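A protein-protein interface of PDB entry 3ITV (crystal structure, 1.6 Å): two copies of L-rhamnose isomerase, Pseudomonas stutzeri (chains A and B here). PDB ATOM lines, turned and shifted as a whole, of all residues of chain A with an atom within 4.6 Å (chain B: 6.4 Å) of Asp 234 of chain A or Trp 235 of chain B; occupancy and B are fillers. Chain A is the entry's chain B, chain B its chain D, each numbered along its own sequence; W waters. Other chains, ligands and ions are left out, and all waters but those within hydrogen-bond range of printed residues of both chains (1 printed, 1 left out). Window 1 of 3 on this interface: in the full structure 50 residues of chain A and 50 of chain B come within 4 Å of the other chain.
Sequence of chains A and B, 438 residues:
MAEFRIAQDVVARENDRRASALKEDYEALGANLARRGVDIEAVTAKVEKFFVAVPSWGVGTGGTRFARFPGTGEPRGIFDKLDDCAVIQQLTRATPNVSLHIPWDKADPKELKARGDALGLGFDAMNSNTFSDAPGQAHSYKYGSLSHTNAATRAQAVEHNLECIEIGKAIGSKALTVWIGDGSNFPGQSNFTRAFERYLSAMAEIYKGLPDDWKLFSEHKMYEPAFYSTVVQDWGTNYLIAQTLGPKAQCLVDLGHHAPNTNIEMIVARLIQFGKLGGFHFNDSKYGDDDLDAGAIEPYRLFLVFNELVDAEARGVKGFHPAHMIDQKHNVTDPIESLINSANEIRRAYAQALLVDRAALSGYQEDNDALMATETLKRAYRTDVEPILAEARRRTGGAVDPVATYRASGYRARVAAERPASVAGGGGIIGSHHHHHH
OE1 of Gln 233 of chain A sits at hydrogen-bond distance from OG1 of Thr 237 of chain A. The backbone NH (N) of Thr 237 of chain A is in hydrogen-bond range of the side-chain carboxylate (OD1) of Asp 234 of chain A. NE2 of Gln 233 of chain B is in hydrogen-bond range of OD2 of Asp 234 of chain B, at 3.2 Å. The side-chain amide oxygen (OE1) of Gln 233 of chain B lies within hydrogen-bond range of the side-chain hydroxyl (OG1) of Thr 237 of chain B, 2.7 Å away. OD1 of Asp 234 of chain B is in hydrogen-bond range of N of Gly 236 of chain B, 3.0 Å away. SG of Cys 251 of chain B lies within hydrogen-bond range of N of Tyr 239 of chain B (3.8 Å).
Hydrophobic or aromatic side chains of chain A within 4 Å of the printed part of chain B: Trp 235 and Leu 240. Among the printed residues, 13 pairs touch across the chains.
Asp 234 of chain A touches Trp 235 of chain B, and with the chains exchanged Trp 235 of chain A touches Asp 234 of chain B. Trp 235 of chain A touches Gly 236 of chain B, and with the chains exchanged Gly 236 of chain A touches Trp 235 of chain B. Trp 235 of chain A touches Thr 237 of chain B, and with the chains exchanged Thr 237 of chain A touches Trp 235 of chain B. Trp 235 of chain A touches Leu 240 of chain B, and with the chains exchanged Leu 240 of chain A touches Trp 235 of chain B. 8 positions are printed for both chains. Of the 13 pairs that touch across the chains among the printed residues, 8 have their exchanged pair printed and touching as well.
Of the printed residues of chain B, Asp 234 of chain A touches Trp 235 and Ile 267. Of chain A, only Asp 234 (2.8 Å), Gly 236 (3.6 Å), Thr 237 (3.4 Å) and Leu 240 (3.9 Å) come within 4 Å of Trp 235 of chain B. Printed residues of chain B within 4 Å of Gly 236 of chain A: Trp 235. Of the printed residues of chain B, Trp 235 of chain A touches Asp 234 (2.8 Å), Gly 236 (3.8 Å), Thr 237 (3.5 Å) and Leu 240 (3.9 Å). Of the printed residues of chain A, Thr 237 of chain B touches Trp 235 (3.5 Å). Thr 262 of chain B touches none of the printed residues of chain A. Val 232 of chain A touches none of the printed residues of chain B.
Among the printed residues, merely in contact across the chains: Gln 233 of chain A with Ile 267 of chain B, Asp 234 of chain A with Ile 267 of chain B, Trp 235 of chain A with Gly 236 of chain B, Trp 235 of chain A with Thr 237 of chain B, Trp 235 of chain A with Leu 240 of chain B, Gly 236 of chain A with Trp 235 of chain B, Thr 237 of chain A with Trp 235 of chain B, Leu 240 of chain A with Trp 235 of chain B and Leu 240 of chain A with Tyr 239 of chain B.
Water W1 bridges OD2 of Asp 234 of chain A (3.3 Å) and OD2 of Asp 234 of chain B (3.4 Å).
The side-chain amide nitrogen (NE2) of Gln 233 of chain A sits close to the side-chain sulfur (SD) of Met 266 of chain B (3.5 Å). The indole nitrogen (NE1) of Trp 235 of chain B lies within hydrogen-bond range of the side-chain carboxylate (OD2) of Asp 234 of chain A, at 2.8 Å. The indole nitrogen of Trp 235 of chain A lies within hydrogen-bond range of the side-chain carboxylate of Asp 234 of chain B (2.8 Å). OG1 of Thr 237 of chain A lies within hydrogen-bond range of NE of Arg 270 of chain B (3.1 Å).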
ATOM      1  N   HIS A 220      11.092 -27.154  20.492  1.00  0.00           N
ATOM      2  CA  HIS A 220      10.647 -27.137  19.103  1.00  0.00           C
ATOM      3  C   HIS A 220      11.186 -25.929  18.348  1.00  0.00           C
ATOM      4  O   HIS A 220      11.555 -24.917  18.945  1.00  0.00           O
ATOM      5  CB  HIS A 220       9.114 -27.158  19.009  1.00  0.00           C
ATOM      6  CG  HIS A 220       8.440 -26.002  19.681  1.00  0.00           C
ATOM      7  ND1 HIS A 220       8.008 -26.050  20.989  1.00  0.00           N
ATOM      8  CD2 HIS A 220       8.109 -24.771  19.221  1.00  0.00           C
ATOM      9  CE1 HIS A 220       7.437 -24.901  21.305  1.00  0.00           C
ATOM     10  NE2 HIS A 220       7.485 -24.108  20.250  1.00  0.00           N
ATOM     11  N   VAL A 232      11.060 -31.834  15.267  1.00  0.00           N
ATOM     12  CA  VAL A 232      10.361 -31.183  16.374  1.00  0.00           C
ATOM     13  C   VAL A 232      10.130 -29.758  15.877  1.00  0.00           C
ATOM     14  O   VAL A 232      10.825 -28.824  16.277  1.00  0.00           O
ATOM     15  CB  VAL A 232      11.226 -31.180  17.658  1.00  0.00           C
ATOM     16  CG1 VAL A 232      10.390 -30.722  18.841  1.00  0.00           C
ATOM     17  CG2 VAL A 232      11.784 -32.578  17.912  1.00  0.00           C
ATOM     18  N   GLN A 233       9.136 -29.605  15.001  1.00  0.00           N
ATOM     19  CA  GLN A 233       8.852 -28.317  14.371  1.00  0.00           C
ATOM     20  C   GLN A 233       7.972 -27.318  15.118  1.00  0.00           C
ATOM     21  O   GLN A 233       8.134 -26.114  14.942  1.00  0.00           O
ATOM     22  CB  GLN A 233       8.288 -28.551  12.954  1.00  0.00           C
ATOM     23  CG  GLN A 233       6.764 -28.447  12.812  1.00  0.00           C
ATOM     24  CD  GLN A 233       6.007 -29.639  13.374  1.00  0.00           C
ATOM     25  OE1 GLN A 233       6.486 -30.304  14.292  1.00  0.00           O
ATOM     26  NE2 GLN A 233       4.814 -29.895  12.845  1.00  0.00           N
ATOM     27  N   ASP A 234       7.036 -27.796  15.931  1.00  0.00           N
ATOM     28  CA  ASP A 234       6.182 -26.876  16.671  1.00  0.00           C
ATOM     29  C   ASP A 234       5.735 -27.437  18.009  1.00  0.00           C
ATOM     30  O   ASP A 234       6.119 -28.550  18.383  1.00  0.00           O
ATOM     31  CB  ASP A 234       4.963 -26.436  15.836  1.00  0.00           C
ATOM     32  CG  ASP A 234       4.057 -27.587  15.438  1.00  0.00           C
ATOM     33  OD1 ASP A 234       4.059 -28.641  16.103  1.00  0.00           O
ATOM     34  OD2 ASP A 234       3.313 -27.418  14.448  1.00  0.00           O
ATOM     35  N   TRP A 235       4.925 -26.668  18.732  1.00  0.00           N
ATOM     36  CA  TRP A 235       4.474 -27.093  20.048  1.00  0.00           C
ATOM     37  C   TRP A 235       3.532 -28.290  20.019  1.00  0.00           C
ATOM     38  O   TRP A 235       3.391 -28.988  21.023  1.00  0.00           O
ATOM     39  CB  TRP A 235       3.815 -25.931  20.800  1.00  0.00           C
ATOM     40  CG  TRP A 235       2.380 -25.699  20.460  1.00  0.00           C
ATOM     41  CD1 TRP A 235       1.888 -25.032  19.378  1.00  0.00           C
ATOM     42  CD2 TRP A 235       1.247 -26.135  21.217  1.00  0.00           C
ATOM     43  NE1 TRP A 235       0.511 -25.023  19.415  1.00  0.00           N
ATOM     44  CE2 TRP A 235       0.093 -25.693  20.534  1.00  0.00           C
ATOM     45  CE3 TRP A 235       1.094 -26.857  22.408  1.00  0.00           C
ATOM     46  CZ2 TRP A 235      -1.202 -25.948  21.002  1.00  0.00           C
ATOM     47  CZ3 TRP A 235      -0.194 -27.113  22.874  1.00  0.00           C
ATOM     48  CH2 TRP A 235      -1.325 -26.656  22.170  1.00  0.00           C
ATOM     49  N   GLY A 236       2.890 -28.520  18.878  1.00  0.00           N
ATOM     50  CA  GLY A 236       1.993 -29.654  18.747  1.00  0.00           C
ATOM     51  C   GLY A 236       2.806 -30.932  18.820  1.00  0.00           C
ATOM     52  O   GLY A 236       2.486 -31.855  19.571  1.00  0.00           O
ATOM     53  N   THR A 237       3.867 -30.991  18.024  1.00  0.00           N
ATOM     54  CA  THR A 237       4.739 -32.155  18.031  1.00  0.00           C
ATOM     55  C   THR A 237       5.421 -32.237  19.392  1.00  0.00           C
ATOM     56  O   THR A 237       5.591 -33.323  19.944  1.00  0.00           O
ATOM     57  CB  THR A 237       5.808 -32.053  16.927  1.00  0.00           C
ATOM     58  OG1 THR A 237       5.177 -32.188  15.650  1.00  0.00           O
ATOM     59  CG2 THR A 237       6.853 -33.149  17.084  1.00  0.00           C
ATOM     60  N   ASN A 238       5.794 -31.084  19.938  1.00  0.00           N
ATOM     61  CA  ASN A 238       6.455 -31.049  21.235  1.00  0.00           C
ATOM     62  C   ASN A 238       5.550 -31.657  22.306  1.00  0.00           C
ATOM     63  O   ASN A 238       6.010 -32.418  23.160  1.00  0.00           O
ATOM     64  CB  ASN A 238       6.832 -29.611  21.610  1.00  0.00           C
ATOM     65  CG  ASN A 238       8.098 -29.545  22.443  1.00  0.00           C
ATOM     66  OD1 ASN A 238       8.623 -30.580  22.855  1.00  0.00           O
ATOM     67  ND2 ASN A 238       8.593 -28.340  22.694  1.00  0.00           N
ATOM     68  N   LEU A 240       3.202 -33.882  21.856  1.00  0.00           N
ATOM     69  CA  LEU A 240       3.136 -35.320  21.612  1.00  0.00           C
ATOM     70  C   LEU A 240       4.366 -36.006  22.202  1.00  0.00           C
ATOM     71  O   LEU A 240       4.277 -37.110  22.743  1.00  0.00           O
ATOM     72  CB  LEU A 240       3.045 -35.604  20.107  1.00  0.00           C
ATOM     73  CG  LEU A 240       1.761 -35.141  19.407  1.00  0.00           C
ATOM     74  CD1 LEU A 240       1.880 -35.414  17.915  1.00  0.00           C
ATOM     75  CD2 LEU A 240       0.549 -35.865  19.983  1.00  0.00           C
ATOM     76  N   HIS B 220      -9.609 -26.430  13.145  1.00  0.00           N
ATOM     77  CA  HIS B 220      -8.820 -25.320  13.665  1.00  0.00           C
ATOM     78  C   HIS B 220      -8.630 -24.223  12.621  1.00  0.00           C
ATOM     79  O   HIS B 220      -8.747 -24.462  11.418  1.00  0.00           O
ATOM     80  CB  HIS B 220      -7.446 -25.805  14.162  1.00  0.00           C
ATOM     81  CG  HIS B 220      -6.594 -26.444  13.103  1.00  0.00           C
ATOM     82  ND1 HIS B 220      -6.604 -27.800  12.854  1.00  0.00           N
ATOM     83  CD2 HIS B 220      -5.698 -25.911  12.237  1.00  0.00           C
ATOM     84  CE1 HIS B 220      -5.752 -28.076  11.882  1.00  0.00           C
ATOM     85  NE2 HIS B 220      -5.188 -26.947  11.490  1.00  0.00           N
ATOM     86  N   GLN B 233      -7.198 -22.564  17.548  1.00  0.00           N
ATOM     87  CA  GLN B 233      -6.284 -21.877  16.643  1.00  0.00           C
ATOM     88  C   GLN B 233      -5.343 -22.700  15.768  1.00  0.00           C
ATOM     89  O   GLN B 233      -4.981 -22.253  14.682  1.00  0.00           O
ATOM     90  CB  GLN B 233      -5.474 -20.835  17.432  1.00  0.00           C
ATOM     91  CG  GLN B 233      -4.045 -21.242  17.791  1.00  0.00           C
ATOM     92  CD  GLN B 233      -3.958 -22.240  18.935  1.00  0.00           C
ATOM     93  OE1 GLN B 233      -4.888 -23.012  19.157  1.00  0.00           O
ATOM     94  NE2 GLN B 233      -2.837 -22.240  19.646  1.00  0.00           N
ATOM     95  N   ASP B 234      -4.933 -23.877  16.224  1.00  0.00           N
ATOM     96  CA  ASP B 234      -4.035 -24.700  15.415  1.00  0.00           C
ATOM     97  C   ASP B 234      -4.226 -26.189  15.654  1.00  0.00           C
ATOM     98  O   ASP B 234      -5.073 -26.596  16.453  1.00  0.00           O
ATOM     99  CB  ASP B 234      -2.563 -24.310  15.639  1.00  0.00           C
ATOM    100  CG  ASP B 234      -2.107 -24.486  17.078  1.00  0.00           C
ATOM    101  OD1 ASP B 234      -2.677 -25.320  17.806  1.00  0.00           O
ATOM    102  OD2 ASP B 234      -1.146 -23.792  17.477  1.00  0.00           O
ATOM    103  N   TRP B 235      -3.433 -27.001  14.960  1.00  0.00           N
ATOM    104  CA  TRP B 235      -3.565 -28.446  15.078  1.00  0.00           C
ATOM    105  C   TRP B 235      -3.202 -29.011  16.446  1.00  0.00           C
ATOM    106  O   TRP B 235      -3.672 -30.086  16.812  1.00  0.00           O
ATOM    107  CB  TRP B 235      -2.753 -29.151  13.982  1.00  0.00           C
ATOM    108  CG  TRP B 235      -1.292 -29.281  14.266  1.00  0.00           C
ATOM    109  CD1 TRP B 235      -0.330 -28.330  14.095  1.00  0.00           C
ATOM    110  CD2 TRP B 235      -0.625 -30.441  14.778  1.00  0.00           C
ATOM    111  NE1 TRP B 235       0.901 -28.828  14.466  1.00  0.00           N
ATOM    112  CE2 TRP B 235       0.746 -30.122  14.889  1.00  0.00           C
ATOM    113  CE3 TRP B 235      -1.055 -31.720  15.154  1.00  0.00           C
ATOM    114  CZ2 TRP B 235       1.694 -31.037  15.362  1.00  0.00           C
ATOM    115  CZ3 TRP B 235      -0.111 -32.631  15.625  1.00  0.00           C
ATOM    116  CH2 TRP B 235       1.247 -32.283  15.724  1.00  0.00           C
ATOM    117  N   GLY B 236      -2.373 -28.290  17.197  1.00  0.00           N
ATOM    118  CA  GLY B 236      -1.994 -28.746  18.523  1.00  0.00           C
ATOM    119  C   GLY B 236      -3.205 -28.705  19.435  1.00  0.00           C
ATOM    120  O   GLY B 236      -3.503 -29.673  20.139  1.00  0.00           O
ATOM    121  N   THR B 237      -3.904 -27.573  19.430  1.00  0.00           N
ATOM    122  CA  THR B 237      -5.105 -27.434  20.241  1.00  0.00           C
ATOM    123  C   THR B 237      -6.141 -28.426  19.726  1.00  0.00           C
ATOM    124  O   THR B 237      -6.859 -29.050  20.504  1.00  0.00           O
ATOM    125  CB  THR B 237      -5.681 -26.000  20.160  1.00  0.00           C
ATOM    126  OG1 THR B 237      -4.812 -25.100  20.857  1.00  0.00           O
ATOM    127  CG2 THR B 237      -7.073 -25.940  20.792  1.00  0.00           C
ATOM    128  N   ASN B 238      -6.196 -28.586  18.409  1.00  0.00           N
ATOM    129  CA  ASN B 238      -7.146 -29.507  17.800  1.00  0.00           C
ATOM    130  C   ASN B 238      -6.890 -30.935  18.295  1.00  0.00           C
ATOM    131  O   ASN B 238      -7.829 -31.673  18.609  1.00  0.00           O
ATOM    132  CB  ASN B 238      -7.038 -29.433  16.273  1.00  0.00           C
ATOM    133  CG  ASN B 238      -8.361 -29.710  15.583  1.00  0.00           C
ATOM    134  OD1 ASN B 238      -8.464 -29.589  14.359  1.00  0.00           O
ATOM    135  ND2 ASN B 238      -9.371 -30.077  16.357  1.00  0.00           N
ATOM    136  N   TYR B 239      -5.621 -31.325  18.382  1.00  0.00           N
ATOM    137  CA  TYR B 239      -5.297 -32.661  18.866  1.00  0.00           C
ATOM    138  C   TYR B 239      -5.776 -32.826  20.307  1.00  0.00           C
ATOM    139  O   TYR B 239      -6.372 -33.846  20.658  1.00  0.00           O
ATOM    140  CB  TYR B 239      -3.789 -32.927  18.807  1.00  0.00           C
ATOM    141  CG  TYR B 239      -3.431 -34.273  19.392  1.00  0.00           C
ATOM    142  CD1 TYR B 239      -3.707 -35.452  18.699  1.00  0.00           C
ATOM    143  CD2 TYR B 239      -2.895 -34.373  20.674  1.00  0.00           C
ATOM    144  CE1 TYR B 239      -3.459 -36.701  19.275  1.00  0.00           C
ATOM    145  CE2 TYR B 239      -2.645 -35.617  21.258  1.00  0.00           C
ATOM    146  CZ  TYR B 239      -2.931 -36.773  20.552  1.00  0.00           C
ATOM    147  OH  TYR B 239      -2.691 -38.002  21.130  1.00  0.00           O
ATOM    148  N   LEU B 240      -5.511 -31.825  21.142  1.00  0.00           N
ATOM    149  CA  LEU B 240      -5.929 -31.881  22.538  1.00  0.00           C
ATOM    150  C   LEU B 240      -7.441 -32.068  22.627  1.00  0.00           C
ATOM    151  O   LEU B 240      -7.938 -32.787  23.495  1.00  0.00           O
ATOM    152  CB  LEU B 240      -5.514 -30.603  23.273  1.00  0.00           C
ATOM    153  CG  LEU B 240      -4.008 -30.391  23.450  1.00  0.00           C
ATOM    154  CD1 LEU B 240      -3.744 -29.018  24.041  1.00  0.00           C
ATOM    155  CD2 LEU B 240      -3.437 -31.482  24.351  1.00  0.00           C
ATOM    156  N   CYS B 251      -9.677 -34.587  14.048  1.00  0.00           N
ATOM    157  CA  CYS B 251      -9.322 -33.265  13.548  1.00  0.00           C
ATOM    158  C   CYS B 251      -9.491 -33.081  12.053  1.00  0.00           C
ATOM    159  O   CYS B 251      -9.171 -33.966  11.262  1.00  0.00           O
ATOM    160  CB  CYS B 251      -7.870 -32.960  13.908  1.00  0.00           C
ATOM    161  SG  CYS B 251      -7.487 -33.191  15.650  1.00  0.00           S
ATOM    162  N   VAL B 253      -8.411 -30.751   8.833  1.00  0.00           N
ATOM    163  CA  VAL B 253      -7.379 -29.831   8.373  1.00  0.00           C
ATOM    164  C   VAL B 253      -7.807 -29.074   7.120  1.00  0.00           C
ATOM    165  O   VAL B 253      -7.982 -29.670   6.051  1.00  0.00           O
ATOM    166  CB  VAL B 253      -6.067 -30.591   8.052  1.00  0.00           C
ATOM    167  CG1 VAL B 253      -4.988 -29.619   7.580  1.00  0.00           C
ATOM    168  CG2 VAL B 253      -5.599 -31.355   9.281  1.00  0.00           C
ATOM    169  N   HIS B 258      -3.607 -22.058   8.205  1.00  0.00           N
ATOM    170  CA  HIS B 258      -2.344 -22.101   8.926  1.00  0.00           C
ATOM    171  C   HIS B 258      -1.480 -20.855   8.786  1.00  0.00           C
ATOM    172  O   HIS B 258      -1.640 -20.065   7.853  1.00  0.00           O
ATOM    173  CB  HIS B 258      -1.562 -23.343   8.485  1.00  0.00           C
ATOM    174  CG  HIS B 258      -2.349 -24.613   8.596  1.00  0.00           C
ATOM    175  ND1 HIS B 258      -3.249 -25.020   7.634  1.00  0.00           N
ATOM    176  CD2 HIS B 258      -2.429 -25.524   9.595  1.00  0.00           C
ATOM    177  CE1 HIS B 258      -3.851 -26.126   8.035  1.00  0.00           C
ATOM    178  NE2 HIS B 258      -3.372 -26.452   9.223  1.00  0.00           N
ATOM    179  N   THR B 262       3.874 -22.469   7.107  1.00  0.00           N
ATOM    180  CA  THR B 262       3.672 -23.715   7.844  1.00  0.00           C
ATOM    181  C   THR B 262       3.873 -24.937   6.946  1.00  0.00           C
ATOM    182  O   THR B 262       3.500 -24.920   5.773  1.00  0.00           O
ATOM    183  CB  THR B 262       2.236 -23.789   8.416  1.00  0.00           C
ATOM    184  OG1 THR B 262       2.025 -22.706   9.328  1.00  0.00           O
ATOM    185  CG2 THR B 262       2.007 -25.118   9.141  1.00  0.00           C
ATOM    186  N   MET B 266       3.277 -31.945   6.984  1.00  0.00           N
ATOM    187  CA  MET B 266       3.792 -32.589   8.190  1.00  0.00           C
ATOM    188  C   MET B 266       2.677 -32.710   9.221  1.00  0.00           C
ATOM    189  O   MET B 266       2.599 -33.705   9.942  1.00  0.00           O
ATOM    190  CB  MET B 266       4.966 -31.813   8.805  1.00  0.00           C
ATOM    191  CG  MET B 266       5.389 -32.402  10.160  1.00  0.00           C
ATOM    192  SD  MET B 266       6.932 -31.791  10.854  1.00  0.00           S
ATOM    193  CE  MET B 266       8.117 -32.817   9.962  1.00  0.00           C
ATOM    194  N   ILE B 267       1.816 -31.697   9.299  1.00  0.00           N
ATOM    195  CA  ILE B 267       0.702 -31.739  10.243  1.00  0.00           C
ATOM    196  C   ILE B 267      -0.165 -32.945   9.897  1.00  0.00           C
ATOM    197  O   ILE B 267      -0.619 -33.679  10.777  1.00  0.00           O
ATOM    198  CB  ILE B 267      -0.157 -30.452  10.164  1.00  0.00           C
ATOM    199  CG1 ILE B 267       0.677 -29.245  10.603  1.00  0.00           C
ATOM    200  CG2 ILE B 267      -1.418 -30.606  11.003  1.00  0.00           C
ATOM    201  CD1 ILE B 267       1.588 -29.510  11.772  1.00  0.00           C
ATOM    202  N   ARG B 270       1.494 -36.110  11.094  1.00  0.00           N
ATOM    203  CA  ARG B 270       1.426 -36.226  12.549  1.00  0.00           C
ATOM    204  C   ARG B 270       0.058 -36.705  13.023  1.00  0.00           C
ATOM    205  O   ARG B 270      -0.037 -37.607  13.858  1.00  0.00           O
ATOM    206  CB  ARG B 270       1.757 -34.881  13.205  1.00  0.00           C
ATOM    207  CG  ARG B 270       3.215 -34.433  13.052  1.00  0.00           C
ATOM    208  CD  ARG B 270       4.143 -35.185  13.999  1.00  0.00           C
ATOM    209  NE  ARG B 270       5.526 -34.713  13.918  1.00  0.00           N
ATOM    210  CZ  ARG B 270       6.431 -35.181  13.063  1.00  0.00           C
ATOM    211  NH1 ARG B 270       6.108 -36.144  12.207  1.00  0.00           N
ATOM    212  NH2 ARG B 270       7.664 -34.688  13.066  1.00  0.00           N
ATOM    213  N   LEU B 271      -1.003 -36.105  12.492  1.00  0.00           N
ATOM    214  CA  LEU B 271      -2.352 -36.498  12.884  1.00  0.00           C
ATOM    215  C   LEU B 271      -2.648 -37.939  12.480  1.00  0.00           C
ATOM    216  O   LEU B 271      -3.338 -38.661  13.199  1.00  0.00           O
ATOM    217  CB  LEU B 271      -3.380 -35.537  12.279  1.00  0.00           C
ATOM    218  CG  LEU B 271      -3.396 -34.153  12.942  1.00  0.00           C
ATOM    219  CD1 LEU B 271      -4.253 -33.196  12.128  1.00  0.00           C
ATOM    220  CD2 LEU B 271      -3.920 -34.270  14.373  1.00  0.00           C
HETATM  221  O   HOH W   1       1.306 -25.027  15.465  1.00  0.00           O
